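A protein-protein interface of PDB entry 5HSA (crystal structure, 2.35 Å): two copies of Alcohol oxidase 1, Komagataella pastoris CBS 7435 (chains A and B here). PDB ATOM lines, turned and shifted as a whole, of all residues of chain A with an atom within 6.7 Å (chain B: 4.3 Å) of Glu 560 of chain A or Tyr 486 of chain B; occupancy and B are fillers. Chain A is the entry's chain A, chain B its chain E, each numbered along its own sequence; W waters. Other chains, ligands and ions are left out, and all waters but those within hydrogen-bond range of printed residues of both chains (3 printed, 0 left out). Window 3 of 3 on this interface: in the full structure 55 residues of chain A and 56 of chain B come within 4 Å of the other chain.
The side-chain hydroxyl (OG) of Ser 517 of chain B lies within hydrogen-bond range of the side-chain carboxylate (OE2) of Glu 563 of chain A, 2.7 Å away.
The backbone carbonyl oxygen of Asn 78 of chain A sits at hydrogen-bond distance from the side-chain hydroxyl of Ser 487 of chain B, at 2.8 Å.
The side-chain hydroxyl (OG) of Ser 517 of chain B lies within hydrogen-bond range of the guanidinium group (NH2) of Arg 80 of chain A, at 3.1 Å.
The side-chain hydroxyl (OG) of Ser 487 of chain B lies close to the backbone carbonyl oxygen (O) of Gly 79 of chain A, 3.5 Å away.
ND1 of His 561 of chain A is in hydrogen-bond range of O of Ser 517 of chain B (3.2 Å).
Printed residues of chain B within 4 Å of Asn 78 of chain A: Ser 487 (2.8 Å).
Of chain B, only Tyr 486 and Ser 517 come within 4 Å of Glu 560 of chain A.
Printed residues of chain B within 4 Å of His 561 of chain A: Ser 517 (3.2 Å).
Of the printed residues of chain B, Glu 563 of chain A touches Ser 517.
Gln 520 of chain B touches none of the printed residues of chain A.
No position is printed for both chains.
Of the 9 pairs that touch across the chains among the printed residues, none has its exchanged pair printed and touching as well.
Water W3 lies within hydrogen-bond range of the side-chain carboxylate (OE2) of Glu 560 of chain A (2.6 Å) and the backbone NH (N) of Tyr 486 of chain B (2.8 Å).
Water W2 lies within hydrogen-bond range of OE1 of Glu 563 of chain A (2.7 Å), OG of Ser 517 of chain B (3.3 Å) and NH2 of Arg 80 of chain A (3.5 Å).
Water W1 lies within hydrogen-bond range of OG of Ser 517 of chain B (3.2 Å) and NH2 of Arg 80 of chain A (3.3 Å).
Printed residues of chain A that touch a printed residue of chain B: Asn 78, Gly 79, Arg 80, Glu 560, His 561 and Glu 563.
Hydrophobic or aromatic side chains of chain A within 4 Å of the printed part of chain B: His 561.
Among the printed residues, 9 pairs touch across the chains.
Among the printed residues, no Asp or Glu carboxylate lies within 4 Å of a Lys or Arg side-chain nitrogen of the other chain.
Among the printed residues, merely in contact across the chains: Arg 80 of chain A with Tyr 486 of chain B (3.4 Å), Arg 80 of chain A with Ser 487 of chain B (3.5 Å), Glu 560 of chain A with Tyr 486 of chain B (3.8 Å) and Glu 560 of chain A with Ser 517 of chain B (3.8 Å).
O of Arg 559 of chain A lies within hydrogen-bond range of NH1 of Arg 80 of chain A (3.2 Å).
The side-chain hydroxyl of Tyr 486 of chain B is in hydrogen-bond range of the side-chain amide nitrogen of Gln 520 of chain B, 2.8 Å away.
The side-chain hydroxyl of Tyr 486 of chain B lies within hydrogen-bond range of the backbone carbonyl oxygen of Ser 517 of chain B (2.7 Å).
The guanidinium group (NE) of Arg 80 of chain A sits at hydrogen-bond distance from the backbone carbonyl oxygen (O) of Glu 560 of chain A.
The side-chain amide nitrogen (ND2) of Asn 78 of chain A sits at hydrogen-bond distance from the side-chain amide oxygen (OD1) of Asn 556 of chain A, 3.3 Å away.
NH1 of Arg 80 of chain A is in hydrogen-bond range of O of Thr 562 of chain A (2.5 Å).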
ATOM      1  N   HIS A  76     -32.201  23.846 -17.195  1.00  0.00           N
ATOM      2  CA  HIS A  76     -31.167  22.839 -16.988  1.00  0.00           C
ATOM      3  C   HIS A  76     -30.407  22.576 -18.272  1.00  0.00           C
ATOM      4  O   HIS A  76     -29.286  22.078 -18.247  1.00  0.00           O
ATOM      5  CB  HIS A  76     -31.790  21.550 -16.453  1.00  0.00           C
ATOM      6  CG  HIS A  76     -32.684  21.769 -15.274  1.00  0.00           C
ATOM      7  ND1 HIS A  76     -34.061  21.802 -15.378  1.00  0.00           N
ATOM      8  CD2 HIS A  76     -32.401  22.009 -13.972  1.00  0.00           C
ATOM      9  CE1 HIS A  76     -34.584  22.034 -14.188  1.00  0.00           C
ATOM     10  NE2 HIS A  76     -33.599  22.163 -13.317  1.00  0.00           N
ATOM     11  N   LEU A  77     -31.032  22.921 -19.394  1.00  0.00           N
ATOM     12  CA  LEU A  77     -30.391  22.857 -20.702  1.00  0.00           C
ATOM     13  C   LEU A  77     -30.045  24.265 -21.197  1.00  0.00           C
ATOM     14  O   LEU A  77     -30.015  24.525 -22.400  1.00  0.00           O
ATOM     15  CB  LEU A  77     -31.306  22.147 -21.699  1.00  0.00           C
ATOM     16  CG  LEU A  77     -31.769  20.758 -21.251  1.00  0.00           C
ATOM     17  CD1 LEU A  77     -32.661  20.121 -22.298  1.00  0.00           C
ATOM     18  CD2 LEU A  77     -30.575  19.868 -20.948  1.00  0.00           C
ATOM     19  N   ASN A  78     -29.809  25.167 -20.248  1.00  0.00           N
ATOM     20  CA  ASN A  78     -29.506  26.570 -20.528  1.00  0.00           C
ATOM     21  C   ASN A  78     -30.498  27.231 -21.482  1.00  0.00           C
ATOM     22  O   ASN A  78     -30.106  27.994 -22.372  1.00  0.00           O
ATOM     23  CB  ASN A  78     -28.082  26.695 -21.077  1.00  0.00           C
ATOM     24  CG  ASN A  78     -27.033  26.438 -20.018  1.00  0.00           C
ATOM     25  OD1 ASN A  78     -27.363  26.171 -18.863  1.00  0.00           O
ATOM     26  ND2 ASN A  78     -25.761  26.513 -20.403  1.00  0.00           N
ATOM     27  N   GLY A  79     -31.780  26.928 -21.295  1.00  0.00           N
ATOM     28  CA  GLY A  79     -32.837  27.576 -22.049  1.00  0.00           C
ATOM     29  C   GLY A  79     -33.334  26.803 -23.255  1.00  0.00           C
ATOM     30  O   GLY A  79     -34.334  27.184 -23.865  1.00  0.00           O
ATOM     31  N   ARG A  80     -32.645  25.720 -23.603  1.00  0.00           N
ATOM     32  CA  ARG A  80     -32.979  24.951 -24.804  1.00  0.00           C
ATOM     33  C   ARG A  80     -34.349  24.284 -24.750  1.00  0.00           C
ATOM     34  O   ARG A  80     -34.761  23.762 -23.715  1.00  0.00           O
ATOM     35  CB  ARG A  80     -31.927  23.866 -25.059  1.00  0.00           C
ATOM     36  CG  ARG A  80     -30.614  24.371 -25.594  1.00  0.00           C
ATOM     37  CD  ARG A  80     -29.900  23.268 -26.360  1.00  0.00           C
ATOM     38  NE  ARG A  80     -29.445  22.191 -25.487  1.00  0.00           N
ATOM     39  CZ  ARG A  80     -29.629  20.897 -25.730  1.00  0.00           C
ATOM     40  NH1 ARG A  80     -29.169  19.997 -24.874  1.00  0.00           N
ATOM     41  NH2 ARG A  80     -30.271  20.502 -26.823  1.00  0.00           N
ATOM     42  N   LEU A 483     -16.313  24.875 -24.566  1.00  0.00           N
ATOM     43  CA  LEU A 483     -15.726  26.194 -24.761  1.00  0.00           C
ATOM     44  C   LEU A 483     -14.753  26.541 -23.636  1.00  0.00           C
ATOM     45  O   LEU A 483     -15.015  27.415 -22.817  1.00  0.00           O
ATOM     46  CB  LEU A 483     -16.835  27.245 -24.860  1.00  0.00           C
ATOM     47  CG  LEU A 483     -17.931  26.864 -25.864  1.00  0.00           C
ATOM     48  CD1 LEU A 483     -19.066  27.865 -25.854  1.00  0.00           C
ATOM     49  CD2 LEU A 483     -17.368  26.724 -27.268  1.00  0.00           C
ATOM     50  N   ALA A 553     -16.778  24.691 -18.118  1.00  0.00           N
ATOM     51  CA  ALA A 553     -16.989  24.695 -19.563  1.00  0.00           C
ATOM     52  C   ALA A 553     -17.619  23.386 -20.024  1.00  0.00           C
ATOM     53  O   ALA A 553     -18.515  23.371 -20.873  1.00  0.00           O
ATOM     54  CB  ALA A 553     -15.671  24.937 -20.289  1.00  0.00           C
ATOM     55  N   GLU A 555     -19.427  21.349 -18.176  1.00  0.00           N
ATOM     56  CA  GLU A 555     -20.797  21.290 -17.669  1.00  0.00           C
ATOM     57  C   GLU A 555     -21.764  22.031 -18.591  1.00  0.00           C
ATOM     58  O   GLU A 555     -22.826  21.508 -18.934  1.00  0.00           O
ATOM     59  CB  GLU A 555     -20.879  21.857 -16.250  1.00  0.00           C
ATOM     60  CG  GLU A 555     -20.227  20.968 -15.210  1.00  0.00           C
ATOM     61  CD  GLU A 555     -20.306  21.537 -13.806  1.00  0.00           C
ATOM     62  OE1 GLU A 555     -20.900  22.623 -13.626  1.00  0.00           O
ATOM     63  OE2 GLU A 555     -19.771  20.890 -12.877  1.00  0.00           O
ATOM     64  N   ASN A 556     -21.389  23.240 -19.001  1.00  0.00           N
ATOM     65  CA  ASN A 556     -22.215  24.007 -19.928  1.00  0.00           C
ATOM     66  C   ASN A 556     -22.314  23.326 -21.287  1.00  0.00           C
ATOM     67  O   ASN A 556     -23.340  23.407 -21.958  1.00  0.00           O
ATOM     68  CB  ASN A 556     -21.671  25.428 -20.086  1.00  0.00           C
ATOM     69  CG  ASN A 556     -22.007  26.300 -18.905  1.00  0.00           C
ATOM     70  OD1 ASN A 556     -23.123  26.244 -18.384  1.00  0.00           O
ATOM     71  ND2 ASN A 556     -21.044  27.102 -18.459  1.00  0.00           N
ATOM     72  N   TYR A 557     -21.234  22.657 -21.678  1.00  0.00           N
ATOM     73  CA  TYR A 557     -21.192  21.859 -22.904  1.00  0.00           C
ATOM     74  C   TYR A 557     -22.253  20.755 -22.861  1.00  0.00           C
ATOM     75  O   TYR A 557     -23.001  20.562 -23.819  1.00  0.00           O
ATOM     76  CB  TYR A 557     -19.790  21.279 -23.071  1.00  0.00           C
ATOM     77  CG  TYR A 557     -19.526  20.372 -24.255  1.00  0.00           C
ATOM     78  CD1 TYR A 557     -19.411  20.885 -25.546  1.00  0.00           C
ATOM     79  CD2 TYR A 557     -19.311  19.009 -24.070  1.00  0.00           C
ATOM     80  CE1 TYR A 557     -19.127  20.058 -26.624  1.00  0.00           C
ATOM     81  CE2 TYR A 557     -19.021  18.175 -25.141  1.00  0.00           C
ATOM     82  CZ  TYR A 557     -18.927  18.704 -26.414  1.00  0.00           C
ATOM     83  OH  TYR A 557     -18.631  17.872 -27.479  1.00  0.00           O
ATOM     84  N   ILE A 558     -22.317  20.045 -21.739  1.00  0.00           N
ATOM     85  CA  ILE A 558     -23.306  18.990 -21.545  1.00  0.00           C
ATOM     86  C   ILE A 558     -24.709  19.585 -21.589  1.00  0.00           C
ATOM     87  O   ILE A 558     -25.586  19.056 -22.275  1.00  0.00           O
ATOM     88  CB  ILE A 558     -23.097  18.234 -20.207  1.00  0.00           C
ATOM     89  CG1 ILE A 558     -22.175  17.030 -20.388  1.00  0.00           C
ATOM     90  CG2 ILE A 558     -24.411  17.674 -19.696  1.00  0.00           C
ATOM     91  CD1 ILE A 558     -20.809  17.354 -20.857  1.00  0.00           C
ATOM     92  N   ARG A 559     -24.915  20.694 -20.875  1.00  0.00           N
ATOM     93  CA  ARG A 559     -26.229  21.333 -20.829  1.00  0.00           C
ATOM     94  C   ARG A 559     -26.692  21.772 -22.211  1.00  0.00           C
ATOM     95  O   ARG A 559     -27.882  21.730 -22.521  1.00  0.00           O
ATOM     96  CB  ARG A 559     -26.222  22.539 -19.888  1.00  0.00           C
ATOM     97  CG  ARG A 559     -25.809  22.217 -18.465  1.00  0.00           C
ATOM     98  CD  ARG A 559     -26.184  23.329 -17.496  1.00  0.00           C
ATOM     99  NE  ARG A 559     -27.129  22.818 -16.510  1.00  0.00           N
ATOM    100  CZ  ARG A 559     -26.805  22.443 -15.278  1.00  0.00           C
ATOM    101  NH1 ARG A 559     -25.554  22.551 -14.850  1.00  0.00           N
ATOM    102  NH2 ARG A 559     -27.741  21.975 -14.468  1.00  0.00           N
ATOM    103  N   GLU A 560     -25.746  22.179 -23.048  1.00  0.00           N
ATOM    104  CA  GLU A 560     -26.093  22.770 -24.333  1.00  0.00           C
ATOM    105  C   GLU A 560     -26.140  21.765 -25.481  1.00  0.00           C
ATOM    106  O   GLU A 560     -26.695  22.068 -26.538  1.00  0.00           O
ATOM    107  CB  GLU A 560     -25.113  23.907 -24.657  1.00  0.00           C
ATOM    108  CG  GLU A 560     -25.339  25.138 -23.779  1.00  0.00           C
ATOM    109  CD  GLU A 560     -24.139  26.069 -23.720  1.00  0.00           C
ATOM    110  OE1 GLU A 560     -23.261  25.972 -24.612  1.00  0.00           O
ATOM    111  OE2 GLU A 560     -24.082  26.885 -22.774  1.00  0.00           O
ATOM    112  N   HIS A 561     -25.581  20.575 -25.286  1.00  0.00           N
ATOM    113  CA  HIS A 561     -25.524  19.615 -26.391  1.00  0.00           C
ATOM    114  C   HIS A 561     -25.959  18.193 -26.014  1.00  0.00           C
ATOM    115  O   HIS A 561     -25.802  17.262 -26.801  1.00  0.00           O
ATOM    116  CB  HIS A 561     -24.111  19.607 -26.995  1.00  0.00           C
ATOM    117  CG  HIS A 561     -23.645  20.965 -27.417  1.00  0.00           C
ATOM    118  ND1 HIS A 561     -24.157  21.612 -28.521  1.00  0.00           N
ATOM    119  CD2 HIS A 561     -22.752  21.814 -26.857  1.00  0.00           C
ATOM    120  CE1 HIS A 561     -23.580  22.796 -28.638  1.00  0.00           C
ATOM    121  NE2 HIS A 561     -22.724  22.943 -27.643  1.00  0.00           N
ATOM    122  N   THR A 562     -26.522  18.032 -24.822  1.00  0.00           N
ATOM    123  CA  THR A 562     -27.138  16.761 -24.453  1.00  0.00           C
ATOM    124  C   THR A 562     -28.448  16.584 -25.213  1.00  0.00           C
ATOM    125  O   THR A 562     -29.217  17.528 -25.357  1.00  0.00           O
ATOM    126  CB  THR A 562     -27.401  16.668 -22.941  1.00  0.00           C
ATOM    127  OG1 THR A 562     -26.150  16.572 -22.249  1.00  0.00           O
ATOM    128  CG2 THR A 562     -28.239  15.447 -22.604  1.00  0.00           C
ATOM    129  N   GLU A 563     -28.687  15.374 -25.707  1.00  0.00           N
ATOM    130  CA  GLU A 563     -29.918  15.064 -26.418  1.00  0.00           C
ATOM    131  C   GLU A 563     -30.538  13.764 -25.911  1.00  0.00           C
ATOM    132  O   GLU A 563     -29.917  13.018 -25.147  1.00  0.00           O
ATOM    133  CB  GLU A 563     -29.653  14.941 -27.918  1.00  0.00           C
ATOM    134  CG  GLU A 563     -28.919  16.113 -28.544  1.00  0.00           C
ATOM    135  CD  GLU A 563     -29.852  17.218 -28.999  1.00  0.00           C
ATOM    136  OE1 GLU A 563     -30.963  17.343 -28.435  1.00  0.00           O
ATOM    137  OE2 GLU A 563     -29.468  17.955 -29.932  1.00  0.00           O
ATOM    138  N   PHE B 484     -22.031  33.853 -27.588  1.00  0.00           N
ATOM    139  CA  PHE B 484     -23.222  34.287 -26.868  1.00  0.00           C
ATOM    140  C   PHE B 484     -23.793  33.151 -26.014  1.00  0.00           C
ATOM    141  O   PHE B 484     -23.588  31.977 -26.321  1.00  0.00           O
ATOM    142  CB  PHE B 484     -24.290  34.782 -27.847  1.00  0.00           C
ATOM    143  CG  PHE B 484     -23.867  35.962 -28.673  1.00  0.00           C
ATOM    144  CD1 PHE B 484     -23.793  37.229 -28.115  1.00  0.00           C
ATOM    145  CD2 PHE B 484     -23.564  35.808 -30.015  1.00  0.00           C
ATOM    146  CE1 PHE B 484     -23.408  38.317 -28.877  1.00  0.00           C
ATOM    147  CE2 PHE B 484     -23.185  36.882 -30.777  1.00  0.00           C
ATOM    148  CZ  PHE B 484     -23.106  38.144 -30.207  1.00  0.00           C
ATOM    149  N   PRO B 485     -24.504  33.497 -24.930  1.00  0.00           N
ATOM    150  CA  PRO B 485     -25.249  32.477 -24.177  1.00  0.00           C
ATOM    151  C   PRO B 485     -26.152  31.705 -25.125  1.00  0.00           C
ATOM    152  O   PRO B 485     -26.755  32.335 -25.993  1.00  0.00           O
ATOM    153  CB  PRO B 485     -26.059  33.298 -23.173  1.00  0.00           C
ATOM    154  CG  PRO B 485     -25.250  34.551 -22.985  1.00  0.00           C
ATOM    155  CD  PRO B 485     -24.618  34.837 -24.326  1.00  0.00           C
ATOM    156  N   TYR B 486     -26.237  30.385 -24.970  1.00  0.00           N
ATOM    157  CA  TYR B 486     -26.875  29.534 -25.977  1.00  0.00           C
ATOM    158  C   TYR B 486     -28.258  30.012 -26.406  1.00  0.00           C
ATOM    159  O   TYR B 486     -28.575  30.007 -27.594  1.00  0.00           O
ATOM    160  CB  TYR B 486     -26.982  28.085 -25.483  1.00  0.00           C
ATOM    161  CG  TYR B 486     -27.299  27.122 -26.610  1.00  0.00           C
ATOM    162  CD1 TYR B 486     -28.606  26.940 -27.049  1.00  0.00           C
ATOM    163  CD2 TYR B 486     -26.289  26.418 -27.253  1.00  0.00           C
ATOM    164  CE1 TYR B 486     -28.900  26.081 -28.085  1.00  0.00           C
ATOM    165  CE2 TYR B 486     -26.576  25.546 -28.290  1.00  0.00           C
ATOM    166  CZ  TYR B 486     -27.885  25.385 -28.700  1.00  0.00           C
ATOM    167  OH  TYR B 486     -28.184  24.529 -29.727  1.00  0.00           O
ATOM    168  N   SER B 487     -29.074  30.420 -25.445  1.00  0.00           N
ATOM    169  CA  SER B 487     -30.458  30.786 -25.736  1.00  0.00           C
ATOM    170  C   SER B 487     -30.681  32.297 -25.832  1.00  0.00           C
ATOM    171  O   SER B 487     -31.822  32.767 -25.833  1.00  0.00           O
ATOM    172  CB  SER B 487     -31.385  30.193 -24.676  1.00  0.00           C
ATOM    173  OG  SER B 487     -31.387  28.781 -24.764  1.00  0.00           O
ATOM    174  N   SER B 488     -29.596  33.054 -25.902  1.00  0.00           N
ATOM    175  CA  SER B 488     -29.705  34.492 -26.099  1.00  0.00           C
ATOM    176  C   SER B 488     -30.336  34.811 -27.453  1.00  0.00           C
ATOM    177  O   SER B 488     -30.098  34.121 -28.445  1.00  0.00           O
ATOM    178  CB  SER B 488     -28.335  35.155 -25.994  1.00  0.00           C
ATOM    179  OG  SER B 488     -28.391  36.485 -26.467  1.00  0.00           O
ATOM    180  N   ARG B 491     -27.820  35.471 -30.226  1.00  0.00           N
ATOM    181  CA  ARG B 491     -26.926  34.401 -30.668  1.00  0.00           C
ATOM    182  C   ARG B 491     -26.783  34.345 -32.190  1.00  0.00           C
ATOM    183  O   ARG B 491     -27.631  34.846 -32.927  1.00  0.00           O
ATOM    184  CB  ARG B 491     -27.418  33.047 -30.150  1.00  0.00           C
ATOM    185  CG  ARG B 491     -28.619  32.495 -30.888  1.00  0.00           C
ATOM    186  CD  ARG B 491     -28.284  31.181 -31.542  1.00  0.00           C
ATOM    187  NE  ARG B 491     -27.990  30.153 -30.553  1.00  0.00           N
ATOM    188  CZ  ARG B 491     -27.066  29.209 -30.700  1.00  0.00           C
ATOM    189  NH1 ARG B 491     -26.887  28.327 -29.730  1.00  0.00           N
ATOM    190  NH2 ARG B 491     -26.322  29.146 -31.798  1.00  0.00           N
ATOM    191  N   SER B 517     -27.362  19.692 -31.518  1.00  0.00           N
ATOM    192  CA  SER B 517     -27.667  21.095 -31.237  1.00  0.00           C
ATOM    193  C   SER B 517     -26.437  21.992 -31.359  1.00  0.00           C
ATOM    194  O   SER B 517     -26.233  22.904 -30.554  1.00  0.00           O
ATOM    195  CB  SER B 517     -28.305  21.231 -29.847  1.00  0.00           C
ATOM    196  OG  SER B 517     -29.588  20.621 -29.815  1.00  0.00           O
ATOM    197  N   THR B 519     -25.816  24.055 -33.857  1.00  0.00           N
ATOM    198  CA  THR B 519     -26.225  25.352 -34.394  1.00  0.00           C
ATOM    199  C   THR B 519     -27.726  25.577 -34.224  1.00  0.00           C
ATOM    200  O   THR B 519     -28.475  24.644 -33.928  1.00  0.00           O
ATOM    201  CB  THR B 519     -25.881  25.499 -35.905  1.00  0.00           C
ATOM    202  OG1 THR B 519     -26.719  24.635 -36.685  1.00  0.00           O
ATOM    203  CG2 THR B 519     -24.411  25.179 -36.179  1.00  0.00           C
ATOM    204  N   GLN B 520     -28.151  26.827 -34.403  1.00  0.00           N
ATOM    205  CA  GLN B 520     -29.570  27.166 -34.451  1.00  0.00           C
ATOM    206  C   GLN B 520     -29.840  27.895 -35.763  1.00  0.00           C
ATOM    207  O   GLN B 520     -29.009  28.684 -36.212  1.00  0.00           O
ATOM    208  CB  GLN B 520     -29.977  28.024 -33.247  1.00  0.00           C
ATOM    209  CG  GLN B 520     -29.921  27.291 -31.908  1.00  0.00           C
ATOM    210  CD  GLN B 520     -30.962  26.177 -31.795  1.00  0.00           C
ATOM    211  OE1 GLN B 520     -32.101  26.325 -32.243  1.00  0.00           O
ATOM    212  NE2 GLN B 520     -30.568  25.055 -31.193  1.00  0.00           N
HETATM  213  O   HOH W   1     -31.844  22.674 -28.798  1.00  0.00           O
HETATM  214  O   HOH W   2     -32.550  19.434 -29.190  1.00  0.00           O
HETATM  215  O   HOH W   3     -24.851  29.376 -22.730  1.00  0.00           O
